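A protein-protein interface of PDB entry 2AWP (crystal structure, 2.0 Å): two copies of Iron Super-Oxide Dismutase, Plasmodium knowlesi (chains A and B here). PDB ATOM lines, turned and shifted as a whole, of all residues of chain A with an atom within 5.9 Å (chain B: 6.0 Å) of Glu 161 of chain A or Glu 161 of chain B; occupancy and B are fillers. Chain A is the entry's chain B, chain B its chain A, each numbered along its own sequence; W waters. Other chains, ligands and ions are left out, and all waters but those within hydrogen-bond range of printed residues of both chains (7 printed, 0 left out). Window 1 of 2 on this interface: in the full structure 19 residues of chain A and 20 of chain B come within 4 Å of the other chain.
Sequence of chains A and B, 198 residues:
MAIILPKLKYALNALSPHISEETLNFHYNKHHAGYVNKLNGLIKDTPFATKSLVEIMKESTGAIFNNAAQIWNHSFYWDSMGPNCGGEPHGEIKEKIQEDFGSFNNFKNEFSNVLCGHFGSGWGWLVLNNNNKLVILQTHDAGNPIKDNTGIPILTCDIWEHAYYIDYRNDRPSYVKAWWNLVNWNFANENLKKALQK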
ATOM      1  N   HIS A  31     -27.755  -0.772  32.733  1.00  0.00           N
ATOM      2  CA  HIS A  31     -29.133  -0.863  32.242  1.00  0.00           C
ATOM      3  C   HIS A  31     -30.010  -1.838  33.044  1.00  0.00           C
ATOM      4  O   HIS A  31     -31.026  -1.429  33.665  1.00  0.00           O
ATOM      5  CB  HIS A  31     -29.189  -1.145  30.721  1.00  0.00           C
ATOM      6  CG  HIS A  31     -28.644  -0.012  29.897  1.00  0.00           C
ATOM      7  ND1 HIS A  31     -29.278   1.211  29.815  1.00  0.00           N
ATOM      8  CD2 HIS A  31     -27.507   0.100  29.165  1.00  0.00           C
ATOM      9  CE1 HIS A  31     -28.559   2.026  29.053  1.00  0.00           C
ATOM     10  NE2 HIS A  31     -27.474   1.380  28.652  1.00  0.00           N
ATOM     11  N   SER A 121     -36.585   1.439  19.599  1.00  0.00           N
ATOM     12  CA  SER A 121     -36.157   0.438  20.585  1.00  0.00           C
ATOM     13  C   SER A 121     -37.125  -0.735  20.578  1.00  0.00           C
ATOM     14  O   SER A 121     -38.349  -0.534  20.465  1.00  0.00           O
ATOM     15  CB  SER A 121     -36.094   1.092  21.975  1.00  0.00           C
ATOM     16  OG  SER A 121     -35.284   2.268  21.934  1.00  0.00           O
ATOM     17  N   ILE A 159     -32.689  -5.370  20.440  1.00  0.00           N
ATOM     18  CA  ILE A 159     -32.207  -4.431  19.430  1.00  0.00           C
ATOM     19  C   ILE A 159     -32.273  -2.940  19.827  1.00  0.00           C
ATOM     20  O   ILE A 159     -32.079  -2.079  18.999  1.00  0.00           O
ATOM     21  CB  ILE A 159     -32.751  -4.714  17.963  1.00  0.00           C
ATOM     22  CG1 ILE A 159     -34.280  -4.831  17.914  1.00  0.00           C
ATOM     23  CG2 ILE A 159     -32.068  -5.967  17.369  1.00  0.00           C
ATOM     24  CD1 ILE A 159     -34.998  -3.468  17.894  1.00  0.00           C
ATOM     25  N   TRP A 160     -32.501  -2.657  21.103  1.00  0.00           N
ATOM     26  CA  TRP A 160     -32.192  -1.333  21.621  1.00  0.00           C
ATOM     27  C   TRP A 160     -30.761  -0.989  21.232  1.00  0.00           C
ATOM     28  O   TRP A 160     -29.883  -1.855  21.251  1.00  0.00           O
ATOM     29  CB  TRP A 160     -32.278  -1.353  23.134  1.00  0.00           C
ATOM     30  CG  TRP A 160     -33.669  -1.298  23.696  1.00  0.00           C
ATOM     31  CD1 TRP A 160     -34.646  -2.233  23.567  1.00  0.00           C
ATOM     32  CD2 TRP A 160     -34.203  -0.269  24.561  1.00  0.00           C
ATOM     33  NE1 TRP A 160     -35.784  -1.840  24.276  1.00  0.00           N
ATOM     34  CE2 TRP A 160     -35.535  -0.641  24.896  1.00  0.00           C
ATOM     35  CE3 TRP A 160     -33.688   0.939  25.078  1.00  0.00           C
ATOM     36  CZ2 TRP A 160     -36.366   0.160  25.715  1.00  0.00           C
ATOM     37  CZ3 TRP A 160     -34.518   1.738  25.890  1.00  0.00           C
ATOM     38  CH2 TRP A 160     -35.834   1.337  26.202  1.00  0.00           C
ATOM     39  N   GLU A 161     -30.532   0.288  20.934  1.00  0.00           N
ATOM     40  CA  GLU A 161     -29.214   0.766  20.541  1.00  0.00           C
ATOM     41  C   GLU A 161     -28.115   0.503  21.547  1.00  0.00           C
ATOM     42  O   GLU A 161     -27.019   0.173  21.135  1.00  0.00           O
ATOM     43  CB  GLU A 161     -29.264   2.241  20.130  1.00  0.00           C
ATOM     44  CG  GLU A 161     -29.997   2.396  18.814  1.00  0.00           C
ATOM     45  CD  GLU A 161     -30.145   3.836  18.359  1.00  0.00           C
ATOM     46  OE1 GLU A 161     -30.303   4.731  19.212  1.00  0.00           O
ATOM     47  OE2 GLU A 161     -30.144   4.042  17.137  1.00  0.00           O
ATOM     48  N   HIS A 162     -28.399   0.634  22.848  1.00  0.00           N
ATOM     49  CA  HIS A 162     -27.404   0.298  23.858  1.00  0.00           C
ATOM     50  C   HIS A 162     -26.885  -1.156  23.815  1.00  0.00           C
ATOM     51  O   HIS A 162     -25.789  -1.390  24.297  1.00  0.00           O
ATOM     52  CB  HIS A 162     -27.877   0.655  25.266  1.00  0.00           C
ATOM     53  CG  HIS A 162     -29.008  -0.179  25.761  1.00  0.00           C
ATOM     54  ND1 HIS A 162     -30.233   0.354  26.092  1.00  0.00           N
ATOM     55  CD2 HIS A 162     -29.117  -1.516  25.956  1.00  0.00           C
ATOM     56  CE1 HIS A 162     -31.035  -0.609  26.505  1.00  0.00           C
ATOM     57  NE2 HIS A 162     -30.379  -1.748  26.425  1.00  0.00           N
ATOM     58  N   ALA A 163     -27.642  -2.092  23.230  1.00  0.00           N
ATOM     59  CA  ALA A 163     -27.191  -3.490  23.033  1.00  0.00           C
ATOM     60  C   ALA A 163     -25.951  -3.631  22.146  1.00  0.00           C
ATOM     61  O   ALA A 163     -25.146  -4.577  22.316  1.00  0.00           O
ATOM     62  CB  ALA A 163     -28.334  -4.371  22.463  1.00  0.00           C
ATOM     63  N   TYR A 164     -25.785  -2.700  21.205  1.00  0.00           N
ATOM     64  CA  TYR A 164     -24.756  -2.871  20.179  1.00  0.00           C
ATOM     65  C   TYR A 164     -23.896  -1.630  19.905  1.00  0.00           C
ATOM     66  O   TYR A 164     -22.796  -1.754  19.304  1.00  0.00           O
ATOM     67  CB  TYR A 164     -25.382  -3.416  18.891  1.00  0.00           C
ATOM     68  CG  TYR A 164     -26.478  -2.556  18.271  1.00  0.00           C
ATOM     69  CD1 TYR A 164     -26.163  -1.534  17.360  1.00  0.00           C
ATOM     70  CD2 TYR A 164     -27.826  -2.775  18.584  1.00  0.00           C
ATOM     71  CE1 TYR A 164     -27.166  -0.733  16.778  1.00  0.00           C
ATOM     72  CE2 TYR A 164     -28.854  -2.015  17.982  1.00  0.00           C
ATOM     73  CZ  TYR A 164     -28.514  -0.979  17.089  1.00  0.00           C
ATOM     74  OH  TYR A 164     -29.519  -0.205  16.503  1.00  0.00           O
ATOM     75  N   TYR A 165     -24.349  -0.460  20.380  1.00  0.00           N
ATOM     76  CA  TYR A 165     -23.768   0.786  19.900  1.00  0.00           C
ATOM     77  C   TYR A 165     -22.268   0.902  20.197  1.00  0.00           C
ATOM     78  O   TYR A 165     -21.523   1.545  19.431  1.00  0.00           O
ATOM     79  CB  TYR A 165     -24.532   2.041  20.372  1.00  0.00           C
ATOM     80  CG  TYR A 165     -24.555   3.081  19.281  1.00  0.00           C
ATOM     81  CD1 TYR A 165     -25.435   2.943  18.209  1.00  0.00           C
ATOM     82  CD2 TYR A 165     -23.674   4.173  19.290  1.00  0.00           C
ATOM     83  CE1 TYR A 165     -25.449   3.834  17.145  1.00  0.00           C
ATOM     84  CE2 TYR A 165     -23.696   5.117  18.220  1.00  0.00           C
ATOM     85  CZ  TYR A 165     -24.582   4.916  17.156  1.00  0.00           C
ATOM     86  OH  TYR A 165     -24.613   5.766  16.095  1.00  0.00           O
ATOM     87  N   ILE A 166     -21.818   0.301  21.309  1.00  0.00           N
ATOM     88  CA  ILE A 166     -20.413   0.409  21.700  1.00  0.00           C
ATOM     89  C   ILE A 166     -19.554  -0.345  20.691  1.00  0.00           C
ATOM     90  O   ILE A 166     -18.434   0.083  20.357  1.00  0.00           O
ATOM     91  CB  ILE A 166     -20.131  -0.133  23.132  1.00  0.00           C
ATOM     92  CG1 ILE A 166     -20.856   0.726  24.184  1.00  0.00           C
ATOM     93  CG2 ILE A 166     -18.606  -0.142  23.418  1.00  0.00           C
ATOM     94  CD1 ILE A 166     -20.999   0.018  25.576  1.00  0.00           C
ATOM     95  N   ARG A 169     -21.660   0.561  16.584  1.00  0.00           N
ATOM     96  CA  ARG A 169     -22.256   1.869  16.306  1.00  0.00           C
ATOM     97  C   ARG A 169     -23.609   1.695  15.586  1.00  0.00           C
ATOM     98  O   ARG A 169     -24.507   1.001  16.092  1.00  0.00           O
ATOM     99  CB  ARG A 169     -21.285   2.775  15.531  1.00  0.00           C
ATOM    100  CG  ARG A 169     -19.953   3.050  16.249  1.00  0.00           C
ATOM    101  CD  ARG A 169     -20.031   4.198  17.245  1.00  0.00           C
ATOM    102  NE  ARG A 169     -18.731   4.556  17.816  1.00  0.00           N
ATOM    103  CZ  ARG A 169     -18.156   3.945  18.850  1.00  0.00           C
ATOM    104  NH1 ARG A 169     -18.754   2.923  19.445  1.00  0.00           N
ATOM    105  NH2 ARG A 169     -16.983   4.371  19.296  1.00  0.00           N
ATOM    106  N   ARG A 172     -26.309  -2.071  13.092  1.00  0.00           N
ATOM    107  CA  ARG A 172     -27.108  -3.110  13.714  1.00  0.00           C
ATOM    108  C   ARG A 172     -27.011  -4.473  12.988  1.00  0.00           C
ATOM    109  O   ARG A 172     -27.027  -5.525  13.662  1.00  0.00           O
ATOM    110  CB  ARG A 172     -28.578  -2.691  13.857  1.00  0.00           C
ATOM    111  CG  ARG A 172     -29.367  -3.654  14.770  1.00  0.00           C
ATOM    112  CD  ARG A 172     -30.869  -3.531  14.605  1.00  0.00           C
ATOM    113  NE  ARG A 172     -31.368  -2.254  15.103  1.00  0.00           N
ATOM    114  CZ  ARG A 172     -32.632  -1.856  15.015  1.00  0.00           C
ATOM    115  NH1 ARG A 172     -33.530  -2.652  14.453  1.00  0.00           N
ATOM    116  NH2 ARG A 172     -32.993  -0.667  15.487  1.00  0.00           N
ATOM    117  N   HIS B  31     -26.742   7.988  10.485  1.00  0.00           N
ATOM    118  CA  HIS B  31     -28.172   8.000  10.803  1.00  0.00           C
ATOM    119  C   HIS B  31     -28.993   8.950   9.936  1.00  0.00           C
ATOM    120  O   HIS B  31     -29.893   8.506   9.206  1.00  0.00           O
ATOM    121  CB  HIS B  31     -28.413   8.251  12.326  1.00  0.00           C
ATOM    122  CG  HIS B  31     -27.911   7.138  13.205  1.00  0.00           C
ATOM    123  ND1 HIS B  31     -28.590   5.942  13.358  1.00  0.00           N
ATOM    124  CD2 HIS B  31     -26.781   7.026  13.950  1.00  0.00           C
ATOM    125  CE1 HIS B  31     -27.934   5.172  14.210  1.00  0.00           C
ATOM    126  NE2 HIS B  31     -26.834   5.804  14.585  1.00  0.00           N
ATOM    127  N   GLY B 120     -37.279   4.748  26.177  1.00  0.00           N
ATOM    128  CA  GLY B 120     -37.086   4.326  24.790  1.00  0.00           C
ATOM    129  C   GLY B 120     -36.615   5.477  23.920  1.00  0.00           C
ATOM    130  O   GLY B 120     -36.143   6.505  24.423  1.00  0.00           O
ATOM    131  N   SER B 121     -36.777   5.310  22.609  1.00  0.00           N
ATOM    132  CA  SER B 121     -36.320   6.288  21.608  1.00  0.00           C
ATOM    133  C   SER B 121     -37.280   7.471  21.555  1.00  0.00           C
ATOM    134  O   SER B 121     -38.491   7.256  21.569  1.00  0.00           O
ATOM    135  CB  SER B 121     -36.253   5.611  20.215  1.00  0.00           C
ATOM    136  OG  SER B 121     -35.251   4.575  20.228  1.00  0.00           O
ATOM    137  N   ASP B 158     -32.731  15.469  20.866  1.00  0.00           N
ATOM    138  CA  ASP B 158     -32.838  14.056  20.573  1.00  0.00           C
ATOM    139  C   ASP B 158     -32.366  13.277  21.760  1.00  0.00           C
ATOM    140  O   ASP B 158     -31.264  13.530  22.278  1.00  0.00           O
ATOM    141  CB  ASP B 158     -31.879  13.783  19.437  1.00  0.00           C
ATOM    142  CG  ASP B 158     -32.024  12.427  18.838  1.00  0.00           C
ATOM    143  OD1 ASP B 158     -32.864  11.593  19.212  1.00  0.00           O
ATOM    144  OD2 ASP B 158     -31.223  12.210  17.950  1.00  0.00           O
ATOM    145  N   ILE B 159     -33.187  12.329  22.208  1.00  0.00           N
ATOM    146  CA  ILE B 159     -32.714  11.429  23.250  1.00  0.00           C
ATOM    147  C   ILE B 159     -32.687   9.966  22.826  1.00  0.00           C
ATOM    148  O   ILE B 159     -32.469   9.107  23.672  1.00  0.00           O
ATOM    149  CB  ILE B 159     -33.412  11.637  24.634  1.00  0.00           C
ATOM    150  CG1 ILE B 159     -34.943  11.618  24.541  1.00  0.00           C
ATOM    151  CG2 ILE B 159     -32.882  12.934  25.301  1.00  0.00           C
ATOM    152  CD1 ILE B 159     -35.482  10.234  24.443  1.00  0.00           C
ATOM    153  N   TRP B 160     -32.844   9.677  21.524  1.00  0.00           N
ATOM    154  CA  TRP B 160     -32.445   8.332  21.032  1.00  0.00           C
ATOM    155  C   TRP B 160     -31.035   8.040  21.569  1.00  0.00           C
ATOM    156  O   TRP B 160     -30.195   8.950  21.639  1.00  0.00           O
ATOM    157  CB  TRP B 160     -32.406   8.241  19.517  1.00  0.00           C
ATOM    158  CG  TRP B 160     -33.754   8.143  18.784  1.00  0.00           C
ATOM    159  CD1 TRP B 160     -34.792   9.027  18.839  1.00  0.00           C
ATOM    160  CD2 TRP B 160     -34.137   7.143  17.829  1.00  0.00           C
ATOM    161  NE1 TRP B 160     -35.808   8.622  18.006  1.00  0.00           N
ATOM    162  CE2 TRP B 160     -35.430   7.474  17.371  1.00  0.00           C
ATOM    163  CE3 TRP B 160     -33.540   5.962  17.370  1.00  0.00           C
ATOM    164  CZ2 TRP B 160     -36.137   6.665  16.471  1.00  0.00           C
ATOM    165  CZ3 TRP B 160     -34.224   5.176  16.471  1.00  0.00           C
ATOM    166  CH2 TRP B 160     -35.495   5.542  15.994  1.00  0.00           C
ATOM    167  N   GLU B 161     -30.770   6.775  21.920  1.00  0.00           N
ATOM    168  CA  GLU B 161     -29.447   6.377  22.445  1.00  0.00           C
ATOM    169  C   GLU B 161     -28.232   6.713  21.580  1.00  0.00           C
ATOM    170  O   GLU B 161     -27.191   7.084  22.130  1.00  0.00           O
ATOM    171  CB  GLU B 161     -29.425   4.922  22.901  1.00  0.00           C
ATOM    172  CG  GLU B 161     -30.432   4.673  24.057  1.00  0.00           C
ATOM    173  CD  GLU B 161     -30.498   3.244  24.543  1.00  0.00           C
ATOM    174  OE1 GLU B 161     -30.514   2.315  23.693  1.00  0.00           O
ATOM    175  OE2 GLU B 161     -30.517   3.059  25.794  1.00  0.00           O
ATOM    176  N   HIS B 162     -28.361   6.625  20.257  1.00  0.00           N
ATOM    177  CA  HIS B 162     -27.251   6.990  19.348  1.00  0.00           C
ATOM    178  C   HIS B 162     -26.854   8.452  19.456  1.00  0.00           C
ATOM    179  O   HIS B 162     -25.737   8.810  19.092  1.00  0.00           O
ATOM    180  CB  HIS B 162     -27.534   6.605  17.883  1.00  0.00           C
ATOM    181  CG  HIS B 162     -28.704   7.314  17.273  1.00  0.00           C
ATOM    182  ND1 HIS B 162     -29.821   6.645  16.825  1.00  0.00           N
ATOM    183  CD2 HIS B 162     -28.933   8.629  17.022  1.00  0.00           C
ATOM    184  CE1 HIS B 162     -30.686   7.510  16.336  1.00  0.00           C
ATOM    185  NE2 HIS B 162     -30.167   8.711  16.429  1.00  0.00           N
ATOM    186  N   ALA B 163     -27.737   9.294  20.009  1.00  0.00           N
ATOM    187  CA  ALA B 163     -27.386  10.703  20.185  1.00  0.00           C
ATOM    188  C   ALA B 163     -26.253  10.885  21.215  1.00  0.00           C
ATOM    189  O   ALA B 163     -25.515  11.878  21.143  1.00  0.00           O
ATOM    190  CB  ALA B 163     -28.592  11.532  20.590  1.00  0.00           C
ATOM    191  N   TYR B 164     -26.134   9.973  22.183  1.00  0.00           N
ATOM    192  CA  TYR B 164     -25.185  10.216  23.279  1.00  0.00           C
ATOM    193  C   TYR B 164     -24.287   9.047  23.672  1.00  0.00           C
ATOM    194  O   TYR B 164     -23.293   9.261  24.394  1.00  0.00           O
ATOM    195  CB  TYR B 164     -25.931  10.753  24.514  1.00  0.00           C
ATOM    196  CG  TYR B 164     -27.048   9.831  25.003  1.00  0.00           C
ATOM    197  CD1 TYR B 164     -26.775   8.787  25.897  1.00  0.00           C
ATOM    198  CD2 TYR B 164     -28.358  10.030  24.593  1.00  0.00           C
ATOM    199  CE1 TYR B 164     -27.797   7.929  26.345  1.00  0.00           C
ATOM    200  CE2 TYR B 164     -29.402   9.208  25.049  1.00  0.00           C
ATOM    201  CZ  TYR B 164     -29.110   8.162  25.916  1.00  0.00           C
ATOM    202  OH  TYR B 164     -30.142   7.372  26.361  1.00  0.00           O
ATOM    203  N   TYR B 165     -24.596   7.838  23.170  1.00  0.00           N
ATOM    204  CA  TYR B 165     -23.941   6.586  23.651  1.00  0.00           C
ATOM    205  C   TYR B 165     -22.402   6.512  23.457  1.00  0.00           C
ATOM    206  O   TYR B 165     -21.675   5.895  24.293  1.00  0.00           O
ATOM    207  CB  TYR B 165     -24.650   5.300  23.112  1.00  0.00           C
ATOM    208  CG  TYR B 165     -24.756   4.265  24.222  1.00  0.00           C
ATOM    209  CD1 TYR B 165     -25.791   4.332  25.160  1.00  0.00           C
ATOM    210  CD2 TYR B 165     -23.811   3.244  24.361  1.00  0.00           C
ATOM    211  CE1 TYR B 165     -25.880   3.424  26.227  1.00  0.00           C
ATOM    212  CE2 TYR B 165     -23.917   2.292  25.413  1.00  0.00           C
ATOM    213  CZ  TYR B 165     -24.935   2.422  26.351  1.00  0.00           C
ATOM    214  OH  TYR B 165     -25.039   1.546  27.400  1.00  0.00           O
ATOM    215  N   ILE B 166     -21.909   7.117  22.374  1.00  0.00           N
ATOM    216  CA  ILE B 166     -20.440   7.238  22.125  1.00  0.00           C
ATOM    217  C   ILE B 166     -19.758   8.061  23.236  1.00  0.00           C
ATOM    218  O   ILE B 166     -18.712   7.681  23.786  1.00  0.00           O
ATOM    219  CB  ILE B 166     -20.177   7.900  20.726  1.00  0.00           C
ATOM    220  CG1 ILE B 166     -20.770   7.012  19.631  1.00  0.00           C
ATOM    221  CG2 ILE B 166     -18.656   8.085  20.450  1.00  0.00           C
ATOM    222  CD1 ILE B 166     -20.870   7.683  18.228  1.00  0.00           C
ATOM    223  N   ARG B 169     -22.236   6.947  27.090  1.00  0.00           N
ATOM    224  CA  ARG B 169     -22.776   5.605  27.378  1.00  0.00           C
ATOM    225  C   ARG B 169     -24.222   5.716  27.908  1.00  0.00           C
ATOM    226  O   ARG B 169     -25.049   6.401  27.289  1.00  0.00           O
ATOM    227  CB  ARG B 169     -21.840   4.861  28.351  1.00  0.00           C
ATOM    228  CG  ARG B 169     -20.445   4.629  27.767  1.00  0.00           C
ATOM    229  CD  ARG B 169     -20.472   3.524  26.736  1.00  0.00           C
ATOM    230  NE  ARG B 169     -19.120   3.164  26.310  1.00  0.00           N
ATOM    231  CZ  ARG B 169     -18.505   3.670  25.246  1.00  0.00           C
ATOM    232  NH1 ARG B 169     -19.137   4.559  24.477  1.00  0.00           N
ATOM    233  NH2 ARG B 169     -17.263   3.264  24.933  1.00  0.00           N
ATOM    234  N   ARG B 172     -27.331   9.466  30.135  1.00  0.00           N
ATOM    235  CA  ARG B 172     -28.139  10.462  29.444  1.00  0.00           C
ATOM    236  C   ARG B 172     -28.139  11.798  30.181  1.00  0.00           C
ATOM    237  O   ARG B 172     -28.073  12.826  29.524  1.00  0.00           O
ATOM    238  CB  ARG B 172     -29.597   9.992  29.225  1.00  0.00           C
ATOM    239  CG  ARG B 172     -30.353  10.891  28.243  1.00  0.00           C
ATOM    240  CD  ARG B 172     -31.837  10.630  28.171  1.00  0.00           C
ATOM    241  NE  ARG B 172     -32.153   9.306  27.667  1.00  0.00           N
ATOM    242  CZ  ARG B 172     -33.379   8.798  27.638  1.00  0.00           C
ATOM    243  NH1 ARG B 172     -34.417   9.517  28.087  1.00  0.00           N
ATOM    244  NH2 ARG B 172     -33.568   7.561  27.178  1.00  0.00           N
HETATM  245  O   HOH W   1     -24.825  -1.334  27.043  1.00  0.00           O
HETATM  246  O   HOH W   2     -38.395   3.312  21.012  1.00  0.00           O
HETATM  247  O   HOH W   3     -32.569   2.209  21.833  1.00  0.00           O
HETATM  248  O   HOH W   4     -32.564   4.742  20.794  1.00  0.00           O
HETATM  249  O   HOH W   5     -24.556   8.734  16.375  1.00  0.00           O
HETATM  250  O   HOH W   6     -17.104   5.550  22.500  1.00  0.00           O
HETATM  251  O   HOH W   7     -16.661   2.458  21.589  1.00  0.00           O
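The side-chain carboxylate (OE1) of Glu 161 of chain B is in hydrogen-bond range of the backbone NH (N) of Glu 161 of chain A (3.4 Å).
The side-chain hydroxyl (OH) of Tyr 165 of chain B lies within hydrogen-bond range of a ring nitrogen (NE2) of His 31 of chain A.
The side-chain hydroxyl of Tyr 165 of chain A is in hydrogen-bond range of a ring nitrogen (NE2) of His 31 of chain B.
A ring nitrogen (ND1) of His 162 of chain B sits at hydrogen-bond distance from the side-chain carboxylate of Glu 161 of chain A, at 2.6 Å.
The side-chain hydroxyl (OG) of Ser 121 of chain B sits at hydrogen-bond distance from the side-chain hydroxyl (OG) of Ser 121 of chain A, 2.9 Å away.
OE2 of Glu 161 of chain B lies within hydrogen-bond range of ND1 of His 162 of chain A, 2.7 Å away.
O of Tyr 165 of chain B sits at hydrogen-bond distance from NH1 of Arg 169 of chain B (2.9 Å).
The backbone NH (N) of Trp 160 of chain B lies within hydrogen-bond range of the side-chain carboxylate (OD1) of Asp 158 of chain B (3.0 Å).
The backbone carbonyl oxygen of Ile 166 of chain A lies within hydrogen-bond range of the guanidinium group of Arg 169 of chain A (3.0 Å).
The backbone carbonyl oxygen of Tyr 165 of chain A sits at hydrogen-bond distance from the guanidinium group of Arg 169 of chain A (3.1 Å).
NH1 of Arg 169 of chain B is in hydrogen-bond range of O of Ile 166 of chain B, at 3.2 Å.
His 31 of chain A touches Glu 161 of chain B (CE1 to OE2, 3.9 Å).
OG of Ser 121 of chain A touches CA of Gly 120 of chain B, 3.95 Å away.
Gly 120 of chain B touches Trp 160 of chain A (CA to CH2, 3.5 Å).
Trp 160 of chain A touches Glu 161 of chain B.
OE2 of Glu 161 of chain A touches CE1 of His 31 of chain B, at 3.8 Å.
Glu 161 of chain A touches Trp 160 of chain B (OE2 to CE3, 3.9 Å).
Tyr 165 of chain B touches His 162 of chain A (CE1 to CB, 3.5 Å).
CB of His 162 of chain B touches CZ of Tyr 165 of chain A (3.5 Å).
CE2 of Tyr 165 of chain B touches CG1 of Ile 166 of chain A, 3.7 Å away.
Arg 169 of chain A touches Ile 166 of chain B.
Of the printed residues of chain B, His 31 of chain A touches Glu 161 and Tyr 165.
Printed residues of chain B within 4 Å of Ser 121 of chain A: Gly 120 (3.95 Å) and Ser 121 (2.9 Å).
Glu 161 of chain A touches just these residues of chain B: His 31, Trp 160, Glu 161 and His 162.
Of the printed residues of chain A, His 31 of chain B touches Glu 161 and Tyr 165.
Of the printed residues of chain A, Gly 120 of chain B touches Ser 121 (3.95 Å) and Trp 160 (3.5 Å).
Of the printed residues of chain A, Glu 161 of chain B touches His 31, Trp 160, Glu 161 and His 162.
Of the printed residues of chain A, Ile 166 of chain B touches Tyr 165 (3.8 Å) and Arg 169 (3.7 Å).
The nearest residue of chain B that does not touch Glu 161 of chain A is Ser 121 of chain B (5.1 Å).
Of the 12 printed residues of chain A, 8 touch a printed residue of chain B.
Hydrophobic or aromatic side chains of chain A that line the printed part of chain B: His 31, Trp 160, His 162, Tyr 165 and Ile 166.
Among the printed residues, 18 pairs touch across the chains.
Among the printed residues, no Asp or Glu carboxylate lies within 4 Å of a Lys or Arg side-chain nitrogen of the other chain.
His 31 of chain A touches Glu 161 of chain B, and with the chains exchanged Glu 161 of chain A touches His 31 of chain B.
Trp 160 of chain A touches Glu 161 of chain B, and with the chains exchanged Glu 161 of chain A touches Trp 160 of chain B.
His 162 of chain A touches Tyr 165 of chain B, and with the chains exchanged Tyr 165 of chain A touches His 162 of chain B.
Tyr 165 of chain A touches Ile 166 of chain B, and with the chains exchanged Ile 166 of chain A touches Tyr 165 of chain B.
Positions printed for both chains: 31, 121, 159, 160, 161, 162, 163, 164, 165, 166, 169 and 172.
Of the 18 pairs that touch across the chains among the printed residues, 16 have their exchanged pair printed and touching as well.
Water W3 lies within hydrogen-bond range of OG of Ser 121 of chain A (2.7 Å), OE1 of Glu 161 of chain B (2.8 Å) and N of Glu 161 of chain A (2.9 Å).
Water W1 bridges OH of Tyr 165 of chain B (2.9 Å) and O of His 162 of chain A (2.9 Å).
Water W5 bridges the backbone carbonyl oxygen of His 162 of chain B (3.0 Å) and the side-chain hydroxyl of Tyr 165 of chain A (3.0 Å).
Water W6 lies within hydrogen-bond range of the backbone carbonyl oxygen of Ile 166 of chain B (3.0 Å), the guanidinium group of Arg 169 of chain B (3.0 Å) and the guanidinium group of Arg 169 of chain A (3.4 Å).
Water W2 lies within hydrogen-bond range of N of Ser 121 of chain A and N of Ser 121 of chain B.
Water W7 lies within hydrogen-bond range of the guanidinium group of Arg 169 of chain A, the backbone carbonyl oxygen of Ile 166 of chain A and the guanidinium group of Arg 169 of chain B.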
